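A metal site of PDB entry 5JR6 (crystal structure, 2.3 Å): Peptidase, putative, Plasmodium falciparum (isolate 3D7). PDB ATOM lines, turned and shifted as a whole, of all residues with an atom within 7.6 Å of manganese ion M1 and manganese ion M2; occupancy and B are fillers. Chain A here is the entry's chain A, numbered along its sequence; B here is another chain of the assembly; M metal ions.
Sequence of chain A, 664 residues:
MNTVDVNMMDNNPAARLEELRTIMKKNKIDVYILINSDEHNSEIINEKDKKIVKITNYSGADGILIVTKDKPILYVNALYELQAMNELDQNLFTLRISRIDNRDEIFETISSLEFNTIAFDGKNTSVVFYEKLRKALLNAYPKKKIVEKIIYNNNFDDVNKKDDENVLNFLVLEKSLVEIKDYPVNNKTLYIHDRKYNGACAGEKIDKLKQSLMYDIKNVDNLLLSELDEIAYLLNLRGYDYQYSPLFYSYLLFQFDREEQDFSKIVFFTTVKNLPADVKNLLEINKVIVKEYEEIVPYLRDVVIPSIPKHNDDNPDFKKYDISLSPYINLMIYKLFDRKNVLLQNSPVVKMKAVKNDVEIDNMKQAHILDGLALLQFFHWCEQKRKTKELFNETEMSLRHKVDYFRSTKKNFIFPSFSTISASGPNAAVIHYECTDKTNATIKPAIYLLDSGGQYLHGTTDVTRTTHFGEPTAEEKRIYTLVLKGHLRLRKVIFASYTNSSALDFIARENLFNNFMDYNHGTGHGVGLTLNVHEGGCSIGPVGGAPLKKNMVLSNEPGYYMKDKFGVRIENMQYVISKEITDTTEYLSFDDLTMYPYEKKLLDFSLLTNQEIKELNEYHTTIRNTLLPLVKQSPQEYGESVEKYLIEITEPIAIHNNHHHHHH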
ATOM      1  N   PHE A 418     -14.044 -36.900 -11.122  1.00  0.00           N
ATOM      2  CA  PHE A 418     -13.555 -36.644  -9.791  1.00  0.00           C
ATOM      3  C   PHE A 418     -14.515 -37.350  -8.887  1.00  0.00           C
ATOM      4  O   PHE A 418     -15.553 -37.805  -9.344  1.00  0.00           O
ATOM      5  CB  PHE A 418     -13.476 -35.122  -9.446  1.00  0.00           C
ATOM      6  CG  PHE A 418     -14.786 -34.386  -9.604  1.00  0.00           C
ATOM      7  CD1 PHE A 418     -15.720 -34.332  -8.555  1.00  0.00           C
ATOM      8  CD2 PHE A 418     -15.098 -33.745 -10.785  1.00  0.00           C
ATOM      9  CE1 PHE A 418     -16.926 -33.640  -8.698  1.00  0.00           C
ATOM     10  CE2 PHE A 418     -16.308 -33.034 -10.939  1.00  0.00           C
ATOM     11  CZ  PHE A 418     -17.225 -32.993  -9.881  1.00  0.00           C
ATOM     12  N   ILE A 421     -19.320 -35.382  -4.929  1.00  0.00           N
ATOM     13  CA  ILE A 421     -19.729 -34.819  -3.659  1.00  0.00           C
ATOM     14  C   ILE A 421     -21.242 -34.919  -3.556  1.00  0.00           C
ATOM     15  O   ILE A 421     -21.992 -34.306  -4.319  1.00  0.00           O
ATOM     16  CB  ILE A 421     -19.264 -33.338  -3.522  1.00  0.00           C
ATOM     17  CG1 ILE A 421     -17.751 -33.276  -3.645  1.00  0.00           C
ATOM     18  CG2 ILE A 421     -19.697 -32.773  -2.170  1.00  0.00           C
ATOM     19  CD1 ILE A 421     -17.199 -31.889  -3.895  1.00  0.00           C
ATOM     20  N   LEU A 450     -25.028 -31.666  -4.819  1.00  0.00           N
ATOM     21  CA  LEU A 450     -24.424 -32.670  -5.679  1.00  0.00           C
ATOM     22  C   LEU A 450     -23.427 -32.010  -6.627  1.00  0.00           C
ATOM     23  O   LEU A 450     -23.815 -31.280  -7.537  1.00  0.00           O
ATOM     24  CB  LEU A 450     -25.498 -33.422  -6.473  1.00  0.00           C
ATOM     25  CG  LEU A 450     -24.945 -34.501  -7.406  1.00  0.00           C
ATOM     26  CD1 LEU A 450     -24.524 -35.711  -6.586  1.00  0.00           C
ATOM     27  CD2 LEU A 450     -25.936 -34.946  -8.517  1.00  0.00           C
ATOM     28  N   ASP A 451     -22.149 -32.298  -6.423  1.00  0.00           N
ATOM     29  CA  ASP A 451     -21.079 -31.809  -7.266  1.00  0.00           C
ATOM     30  C   ASP A 451     -20.523 -33.062  -7.970  1.00  0.00           C
ATOM     31  O   ASP A 451     -20.012 -33.968  -7.315  1.00  0.00           O
ATOM     32  CB  ASP A 451     -20.015 -31.100  -6.425  1.00  0.00           C
ATOM     33  CG  ASP A 451     -19.000 -30.329  -7.254  1.00  0.00           C
ATOM     34  OD1 ASP A 451     -19.038 -30.425  -8.503  1.00  0.00           O
ATOM     35  OD2 ASP A 451     -18.168 -29.590  -6.654  1.00  0.00           O
ATOM     36  N   SER A 452     -20.680 -33.151  -9.275  1.00  0.00           N
ATOM     37  CA  SER A 452     -20.322 -34.361  -9.986  1.00  0.00           C
ATOM     38  C   SER A 452     -19.962 -34.052 -11.414  1.00  0.00           C
ATOM     39  O   SER A 452     -20.273 -32.970 -11.924  1.00  0.00           O
ATOM     40  CB  SER A 452     -21.465 -35.375  -9.941  1.00  0.00           C
ATOM     41  OG  SER A 452     -22.501 -34.981 -10.832  1.00  0.00           O
ATOM     42  N   GLY A 453     -19.272 -34.995 -12.056  1.00  0.00           N
ATOM     43  CA  GLY A 453     -18.793 -34.772 -13.417  1.00  0.00           C
ATOM     44  C   GLY A 453     -18.318 -36.045 -14.058  1.00  0.00           C
ATOM     45  O   GLY A 453     -18.158 -37.066 -13.396  1.00  0.00           O
ATOM     46  N   THR A 461     -16.480 -32.904 -17.833  1.00  0.00           N
ATOM     47  CA  THR A 461     -17.560 -32.068 -17.285  1.00  0.00           C
ATOM     48  C   THR A 461     -17.468 -31.941 -15.771  1.00  0.00           C
ATOM     49  O   THR A 461     -16.942 -32.835 -15.091  1.00  0.00           O
ATOM     50  CB  THR A 461     -18.951 -32.618 -17.622  1.00  0.00           C
ATOM     51  OG1 THR A 461     -19.212 -33.791 -16.836  1.00  0.00           O
ATOM     52  CG2 THR A 461     -19.037 -32.975 -19.099  1.00  0.00           C
ATOM     53  N   ASP A 462     -17.906 -30.799 -15.264  1.00  0.00           N
ATOM     54  CA  ASP A 462     -17.970 -30.519 -13.843  1.00  0.00           C
ATOM     55  C   ASP A 462     -19.202 -29.668 -13.532  1.00  0.00           C
ATOM     56  O   ASP A 462     -19.279 -28.532 -13.981  1.00  0.00           O
ATOM     57  CB  ASP A 462     -16.694 -29.789 -13.442  1.00  0.00           C
ATOM     58  CG  ASP A 462     -16.550 -29.585 -11.965  1.00  0.00           C
ATOM     59  OD1 ASP A 462     -15.464 -29.130 -11.586  1.00  0.00           O
ATOM     60  OD2 ASP A 462     -17.486 -29.864 -11.176  1.00  0.00           O
ATOM     61  N   VAL A 463     -20.138 -30.149 -12.718  1.00  0.00           N
ATOM     62  CA  VAL A 463     -21.396 -29.424 -12.521  1.00  0.00           C
ATOM     63  C   VAL A 463     -21.873 -29.587 -11.086  1.00  0.00           C
ATOM     64  O   VAL A 463     -21.814 -30.691 -10.534  1.00  0.00           O
ATOM     65  CB  VAL A 463     -22.514 -29.911 -13.495  1.00  0.00           C
ATOM     66  CG1 VAL A 463     -22.640 -31.447 -13.468  1.00  0.00           C
ATOM     67  CG2 VAL A 463     -23.880 -29.260 -13.140  1.00  0.00           C
ATOM     68  N   THR A 464     -22.332 -28.504 -10.468  1.00  0.00           N
ATOM     69  CA  THR A 464     -22.995 -28.607  -9.176  1.00  0.00           C
ATOM     70  C   THR A 464     -24.392 -28.010  -9.221  1.00  0.00           C
ATOM     71  O   THR A 464     -24.631 -26.982  -9.863  1.00  0.00           O
ATOM     72  CB  THR A 464     -22.199 -27.917  -8.044  1.00  0.00           C
ATOM     73  OG1 THR A 464     -20.817 -28.294  -8.128  1.00  0.00           O
ATOM     74  CG2 THR A 464     -22.750 -28.302  -6.676  1.00  0.00           C
ATOM     75  N   GLY A 522     -12.044 -20.291  -5.038  1.00  0.00           N
ATOM     76  CA  GLY A 522     -12.102 -19.540  -6.282  1.00  0.00           C
ATOM     77  C   GLY A 522     -13.435 -19.726  -6.992  1.00  0.00           C
ATOM     78  O   GLY A 522     -14.201 -20.639  -6.655  1.00  0.00           O
ATOM     79  N   THR A 523     -13.746 -18.833  -7.917  1.00  0.00           N
ATOM     80  CA  THR A 523     -15.018 -18.888  -8.647  1.00  0.00           C
ATOM     81  C   THR A 523     -15.007 -19.810  -9.865  1.00  0.00           C
ATOM     82  O   THR A 523     -16.032 -20.412 -10.217  1.00  0.00           O
ATOM     83  CB  THR A 523     -15.438 -17.465  -9.109  1.00  0.00           C
ATOM     84  OG1 THR A 523     -15.606 -16.624  -7.953  1.00  0.00           O
ATOM     85  CG2 THR A 523     -16.734 -17.498  -9.900  1.00  0.00           C
ATOM     86  N   GLY A 524     -13.868 -19.885 -10.542  1.00  0.00           N
ATOM     87  CA  GLY A 524     -13.768 -20.740 -11.710  1.00  0.00           C
ATOM     88  C   GLY A 524     -12.354 -21.175 -12.017  1.00  0.00           C
ATOM     89  O   GLY A 524     -11.384 -20.469 -11.684  1.00  0.00           O
ATOM     90  N   HIS A 525     -12.247 -22.322 -12.668  1.00  0.00           N
ATOM     91  CA  HIS A 525     -10.990 -22.881 -13.143  1.00  0.00           C
ATOM     92  C   HIS A 525     -11.151 -23.274 -14.604  1.00  0.00           C
ATOM     93  O   HIS A 525     -12.273 -23.514 -15.080  1.00  0.00           O
ATOM     94  CB  HIS A 525     -10.587 -24.095 -12.298  1.00  0.00           C
ATOM     95  CG  HIS A 525     -11.665 -25.130 -12.175  1.00  0.00           C
ATOM     96  ND1 HIS A 525     -11.976 -26.013 -13.190  1.00  0.00           N
ATOM     97  CD2 HIS A 525     -12.509 -25.434 -11.155  1.00  0.00           C
ATOM     98  CE1 HIS A 525     -12.961 -26.814 -12.801  1.00  0.00           C
ATOM     99  NE2 HIS A 525     -13.298 -26.483 -11.572  1.00  0.00           N
ATOM    100  N   GLY A 526     -10.040 -23.359 -15.327  1.00  0.00           N
ATOM    101  CA  GLY A 526     -10.044 -23.922 -16.661  1.00  0.00           C
ATOM    102  C   GLY A 526     -10.335 -25.419 -16.570  1.00  0.00           C
ATOM    103  O   GLY A 526     -10.242 -26.009 -15.483  1.00  0.00           O
ATOM    104  N   VAL A 527     -10.726 -26.032 -17.691  1.00  0.00           N
ATOM    105  CA  VAL A 527     -11.109 -27.436 -17.707  1.00  0.00           C
ATOM    106  C   VAL A 527     -10.604 -28.108 -18.968  1.00  0.00           C
ATOM    107  O   VAL A 527     -10.753 -27.572 -20.067  1.00  0.00           O
ATOM    108  CB  VAL A 527     -12.649 -27.604 -17.586  1.00  0.00           C
ATOM    109  CG1 VAL A 527     -13.085 -29.074 -17.750  1.00  0.00           C
ATOM    110  CG2 VAL A 527     -13.123 -27.064 -16.254  1.00  0.00           C
ATOM    111  N   VAL A 533      -9.994 -32.262 -14.545  1.00  0.00           N
ATOM    112  CA  VAL A 533     -11.118 -31.403 -14.318  1.00  0.00           C
ATOM    113  C   VAL A 533     -10.617 -30.024 -13.892  1.00  0.00           C
ATOM    114  O   VAL A 533     -11.278 -29.030 -14.131  1.00  0.00           O
ATOM    115  CB  VAL A 533     -12.063 -31.994 -13.260  1.00  0.00           C
ATOM    116  CG1 VAL A 533     -11.394 -31.988 -11.873  1.00  0.00           C
ATOM    117  CG2 VAL A 533     -13.379 -31.241 -13.246  1.00  0.00           C
ATOM    118  N   HIS A 534      -9.428 -29.967 -13.293  1.00  0.00           N
ATOM    119  CA  HIS A 534      -8.785 -28.682 -12.982  1.00  0.00           C
ATOM    120  C   HIS A 534      -7.592 -28.471 -13.889  1.00  0.00           C
ATOM    121  O   HIS A 534      -6.566 -29.119 -13.740  1.00  0.00           O
ATOM    122  CB  HIS A 534      -8.349 -28.626 -11.527  1.00  0.00           C
ATOM    123  CG  HIS A 534      -9.499 -28.611 -10.574  1.00  0.00           C
ATOM    124  ND1 HIS A 534      -9.445 -29.204  -9.329  1.00  0.00           N
ATOM    125  CD2 HIS A 534     -10.750 -28.108 -10.683  1.00  0.00           C
ATOM    126  CE1 HIS A 534     -10.594 -29.056  -8.719  1.00  0.00           C
ATOM    127  NE2 HIS A 534     -11.414 -28.396  -9.523  1.00  0.00           N
ATOM    128  N   SER A 555     -15.199 -22.938 -15.425  1.00  0.00           N
ATOM    129  CA  SER A 555     -16.278 -23.175 -14.494  1.00  0.00           C
ATOM    130  C   SER A 555     -16.752 -21.832 -13.912  1.00  0.00           C
ATOM    131  O   SER A 555     -16.048 -20.821 -13.967  1.00  0.00           O
ATOM    132  CB  SER A 555     -15.862 -24.138 -13.373  1.00  0.00           C
ATOM    133  OG  SER A 555     -14.841 -23.633 -12.525  1.00  0.00           O
ATOM    134  N   ASN A 556     -18.001 -21.825 -13.472  1.00  0.00           N
ATOM    135  CA  ASN A 556     -18.608 -20.695 -12.801  1.00  0.00           C
ATOM    136  C   ASN A 556     -19.273 -21.270 -11.582  1.00  0.00           C
ATOM    137  O   ASN A 556     -20.328 -21.881 -11.711  1.00  0.00           O
ATOM    138  CB  ASN A 556     -19.591 -20.073 -13.785  1.00  0.00           C
ATOM    139  CG  ASN A 556     -20.545 -19.091 -13.172  1.00  0.00           C
ATOM    140  OD1 ASN A 556     -20.454 -18.695 -12.004  1.00  0.00           O
ATOM    141  ND2 ASN A 556     -21.477 -18.653 -13.995  1.00  0.00           N
ATOM    142  N   GLU A 557     -18.693 -21.086 -10.410  1.00  0.00           N
ATOM    143  CA  GLU A 557     -19.197 -21.843  -9.274  1.00  0.00           C
ATOM    144  C   GLU A 557     -19.149 -21.109  -7.939  1.00  0.00           C
ATOM    145  O   GLU A 557     -18.477 -21.562  -7.016  1.00  0.00           O
ATOM    146  CB  GLU A 557     -18.449 -23.178  -9.147  1.00  0.00           C
ATOM    147  CG  GLU A 557     -16.925 -23.070  -9.180  1.00  0.00           C
ATOM    148  CD  GLU A 557     -16.239 -24.439  -9.250  1.00  0.00           C
ATOM    149  OE1 GLU A 557     -16.659 -25.373  -8.518  1.00  0.00           O
ATOM    150  OE2 GLU A 557     -15.296 -24.585 -10.075  1.00  0.00           O
ATOM    151  N   ARG A 569     -23.857 -24.496  -3.526  1.00  0.00           N
ATOM    152  CA  ARG A 569     -22.936 -24.137  -4.594  1.00  0.00           C
ATOM    153  C   ARG A 569     -23.681 -24.361  -5.888  1.00  0.00           C
ATOM    154  O   ARG A 569     -24.500 -25.266  -5.992  1.00  0.00           O
ATOM    155  CB  ARG A 569     -21.632 -24.961  -4.518  1.00  0.00           C
ATOM    156  CG  ARG A 569     -20.657 -24.732  -5.708  1.00  0.00           C
ATOM    157  CD  ARG A 569     -19.207 -25.260  -5.428  1.00  0.00           C
ATOM    158  NE  ARG A 569     -19.147 -26.714  -5.233  1.00  0.00           N
ATOM    159  CZ  ARG A 569     -19.036 -27.299  -4.047  1.00  0.00           C
ATOM    160  NH1 ARG A 569     -18.977 -26.556  -2.947  1.00  0.00           N
ATOM    161  NH2 ARG A 569     -18.991 -28.631  -3.951  1.00  0.00           N
ATOM    162  N   GLU A 571     -22.858 -24.505 -10.029  1.00  0.00           N
ATOM    163  CA  GLU A 571     -21.731 -24.533 -10.927  1.00  0.00           C
ATOM    164  C   GLU A 571     -22.093 -24.930 -12.332  1.00  0.00           C
ATOM    165  O   GLU A 571     -22.759 -25.938 -12.559  1.00  0.00           O
ATOM    166  CB  GLU A 571     -20.675 -25.498 -10.410  1.00  0.00           C
ATOM    167  CG  GLU A 571     -19.567 -25.768 -11.389  1.00  0.00           C
ATOM    168  CD  GLU A 571     -18.625 -26.827 -10.869  1.00  0.00           C
ATOM    169  OE1 GLU A 571     -19.033 -27.599  -9.964  1.00  0.00           O
ATOM    170  OE2 GLU A 571     -17.474 -26.859 -11.345  1.00  0.00           O
ATOM    171  N   ASN A 572     -21.651 -24.115 -13.279  1.00  0.00           N
ATOM    172  CA  ASN A 572     -21.718 -24.450 -14.690  1.00  0.00           C
ATOM    173  C   ASN A 572     -20.331 -24.397 -15.258  1.00  0.00           C
ATOM    174  O   ASN A 572     -19.413 -23.820 -14.665  1.00  0.00           O
ATOM    175  CB  ASN A 572     -22.587 -23.471 -15.482  1.00  0.00           C
ATOM    176  CG  ASN A 572     -24.067 -23.686 -15.290  1.00  0.00           C
ATOM    177  OD1 ASN A 572     -24.504 -24.415 -14.385  1.00  0.00           O
ATOM    178  ND2 ASN A 572     -24.858 -23.044 -16.151  1.00  0.00           N
ATOM    179  N   MET A 573     -20.186 -25.002 -16.436  1.00  0.00           N
ATOM    180  CA  MET A 573     -19.051 -24.732 -17.286  1.00  0.00           C
ATOM    181  C   MET A 573     -19.583 -23.958 -18.484  1.00  0.00           C
ATOM    182  O   MET A 573     -20.715 -24.159 -18.910  1.00  0.00           O
ATOM    183  CB  MET A 573     -18.343 -26.043 -17.736  1.00  0.00           C
ATOM    184  CG  MET A 573     -17.419 -26.622 -16.661  1.00  0.00           C
ATOM    185  SD  MET A 573     -16.933 -28.363 -17.073  1.00  0.00           S
ATOM    186  CE  MET A 573     -16.276 -28.106 -18.699  1.00  0.00           C
ATOM    187  CB  01B B   1     -14.208 -30.099  -7.992  1.00  0.00           C
ATOM    188  CA  01B B   1     -14.987 -28.929  -7.481  1.00  0.00           C
ATOM    189  N   01B B   1     -15.073 -30.809  -8.843  1.00  0.00           N
ATOM    190  O2  01B B   1     -16.072 -28.705  -8.351  1.00  0.00           O
ATOM    191  C   01B B   1     -14.154 -27.696  -7.504  1.00  0.00           C
ATOM    192  C6  01B B   1     -13.831 -30.966  -6.794  1.00  0.00           C
ATOM    193  C7  01B B   1     -12.506 -31.762  -7.068  1.00  0.00           C
ATOM    194  C8  01B B   1     -12.086 -31.953  -8.337  1.00  0.00           C
ATOM    195  C9  01B B   1     -10.795 -32.734  -8.619  1.00  0.00           C
ATOM    196  C10 01B B   1     -10.055 -33.243  -7.573  1.00  0.00           C
ATOM    197  C11 01B B   1     -10.527 -33.029  -6.152  1.00  0.00           C
ATOM    198  C12 01B B   1     -11.681 -32.330  -5.900  1.00  0.00           C
ATOM    199  O   01B B   1     -13.347 -27.526  -8.402  1.00  0.00           O
ATOM    200  N   PRO B   2     -14.368 -26.704  -6.451  1.00  0.00           N
ATOM    201  CA  PRO B   2     -13.675 -25.419  -6.290  1.00  0.00           C
ATOM    202  C   PRO B   2     -12.234 -25.424  -6.573  1.00  0.00           C
ATOM    203  O   PRO B   2     -11.510 -26.341  -6.153  1.00  0.00           O
ATOM    204  CB  PRO B   2     -13.910 -25.085  -4.830  1.00  0.00           C
ATOM    205  CG  PRO B   2     -15.214 -25.696  -4.492  1.00  0.00           C
ATOM    206  CD  PRO B   2     -15.320 -26.877  -5.407  1.00  0.00           C
ATOM    207  N   PRO B   3     -11.644 -24.282  -7.346  1.00  0.00           N
ATOM    208  CA  PRO B   3     -10.231 -24.139  -7.682  1.00  0.00           C
ATOM    209  C   PRO B   3      -9.430 -23.926  -6.413  1.00  0.00           C
ATOM    210  O   PRO B   3      -8.293 -24.355  -6.332  1.00  0.00           O
ATOM    211  CB  PRO B   3     -10.158 -22.956  -8.622  1.00  0.00           C
ATOM    212  CG  PRO B   3     -11.497 -22.287  -8.565  1.00  0.00           C
ATOM    213  CD  PRO B   3     -12.401 -23.169  -7.851  1.00  0.00           C
HETATM  214 MN    MN M   1     -15.306 -27.106 -10.394  1.00  0.00          MN
HETATM  215 MN    MN M   2     -17.693 -29.227  -9.321  1.00  0.00          MN
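Manganese ion M1 is bound by OD1 of Asp 462 (2.4 Å), OE2 of Glu 571 (2.4 Å), NE2 of His 525 (2.4 Å) and OE2 of Glu 557 (2.5 Å).
Slightly farther from manganese ion M1 lies O2 of 01B 1 of chain B (2.7 Å).
Slightly farther from manganese ion M1 lies O of 01B 1 of chain B (2.8 Å).
Slightly farther from manganese ion M1 lies the side-chain carboxylate (OE1) of Glu 557 (2.9 Å).
The side-chain carboxylate of Asp 451 lies close to the side-chain hydroxyl of Thr 464 (3.3 Å).
The guanidinium group (NH2) of Arg 569 lies within salt-bridge range of the side-chain carboxylate (OD2) of Asp 451, at 3.0 Å.
A ring nitrogen (NE2) of His 525 sits close to a ring nitrogen (NE2) of His 534, at 3.4 Å.
O of 01B 1 of chain B lies close to NE2 of His 525 (3.3 Å).
The backbone NH of Asp 462 is in hydrogen-bond range of the side-chain sulfur of Met 573 (3.2 Å).
O2 of 01B 1 of chain B sits close to the side-chain carboxylate of Glu 557 (3.4 Å).
O of Asp 451 is in hydrogen-bond range of N of Ile 421 (2.9 Å).
The backbone carbonyl oxygen (O) of Thr 523 lies within hydrogen-bond range of the backbone NH (N) of Glu 557, at 2.8 Å.
Phe 418 touches manganese ion M2.
Thr 464 touches manganese ion M2 (OG1 to MN, 3.5 Å).
Six residues have an atom within 4 Å of manganese ion M2: Phe 418, Asp 451, Asp 462, Thr 464, Glu 571 and 01B 1 of chain B.
The nearest printed residue that does not touch manganese ion M2 is Glu 557 (4.1 Å).
Manganese ion M2 is bound by O2 of 01B 1 of chain B (2.0 Å), OD2 of Asp 462 (2.0 Å), OD1 of Asp 451 (2.0 Å) and OE1 of Glu 571 (2.2 Å).
Slightly farther from manganese ion M2 lies OD2 of Asp 451 (2.7 Å).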
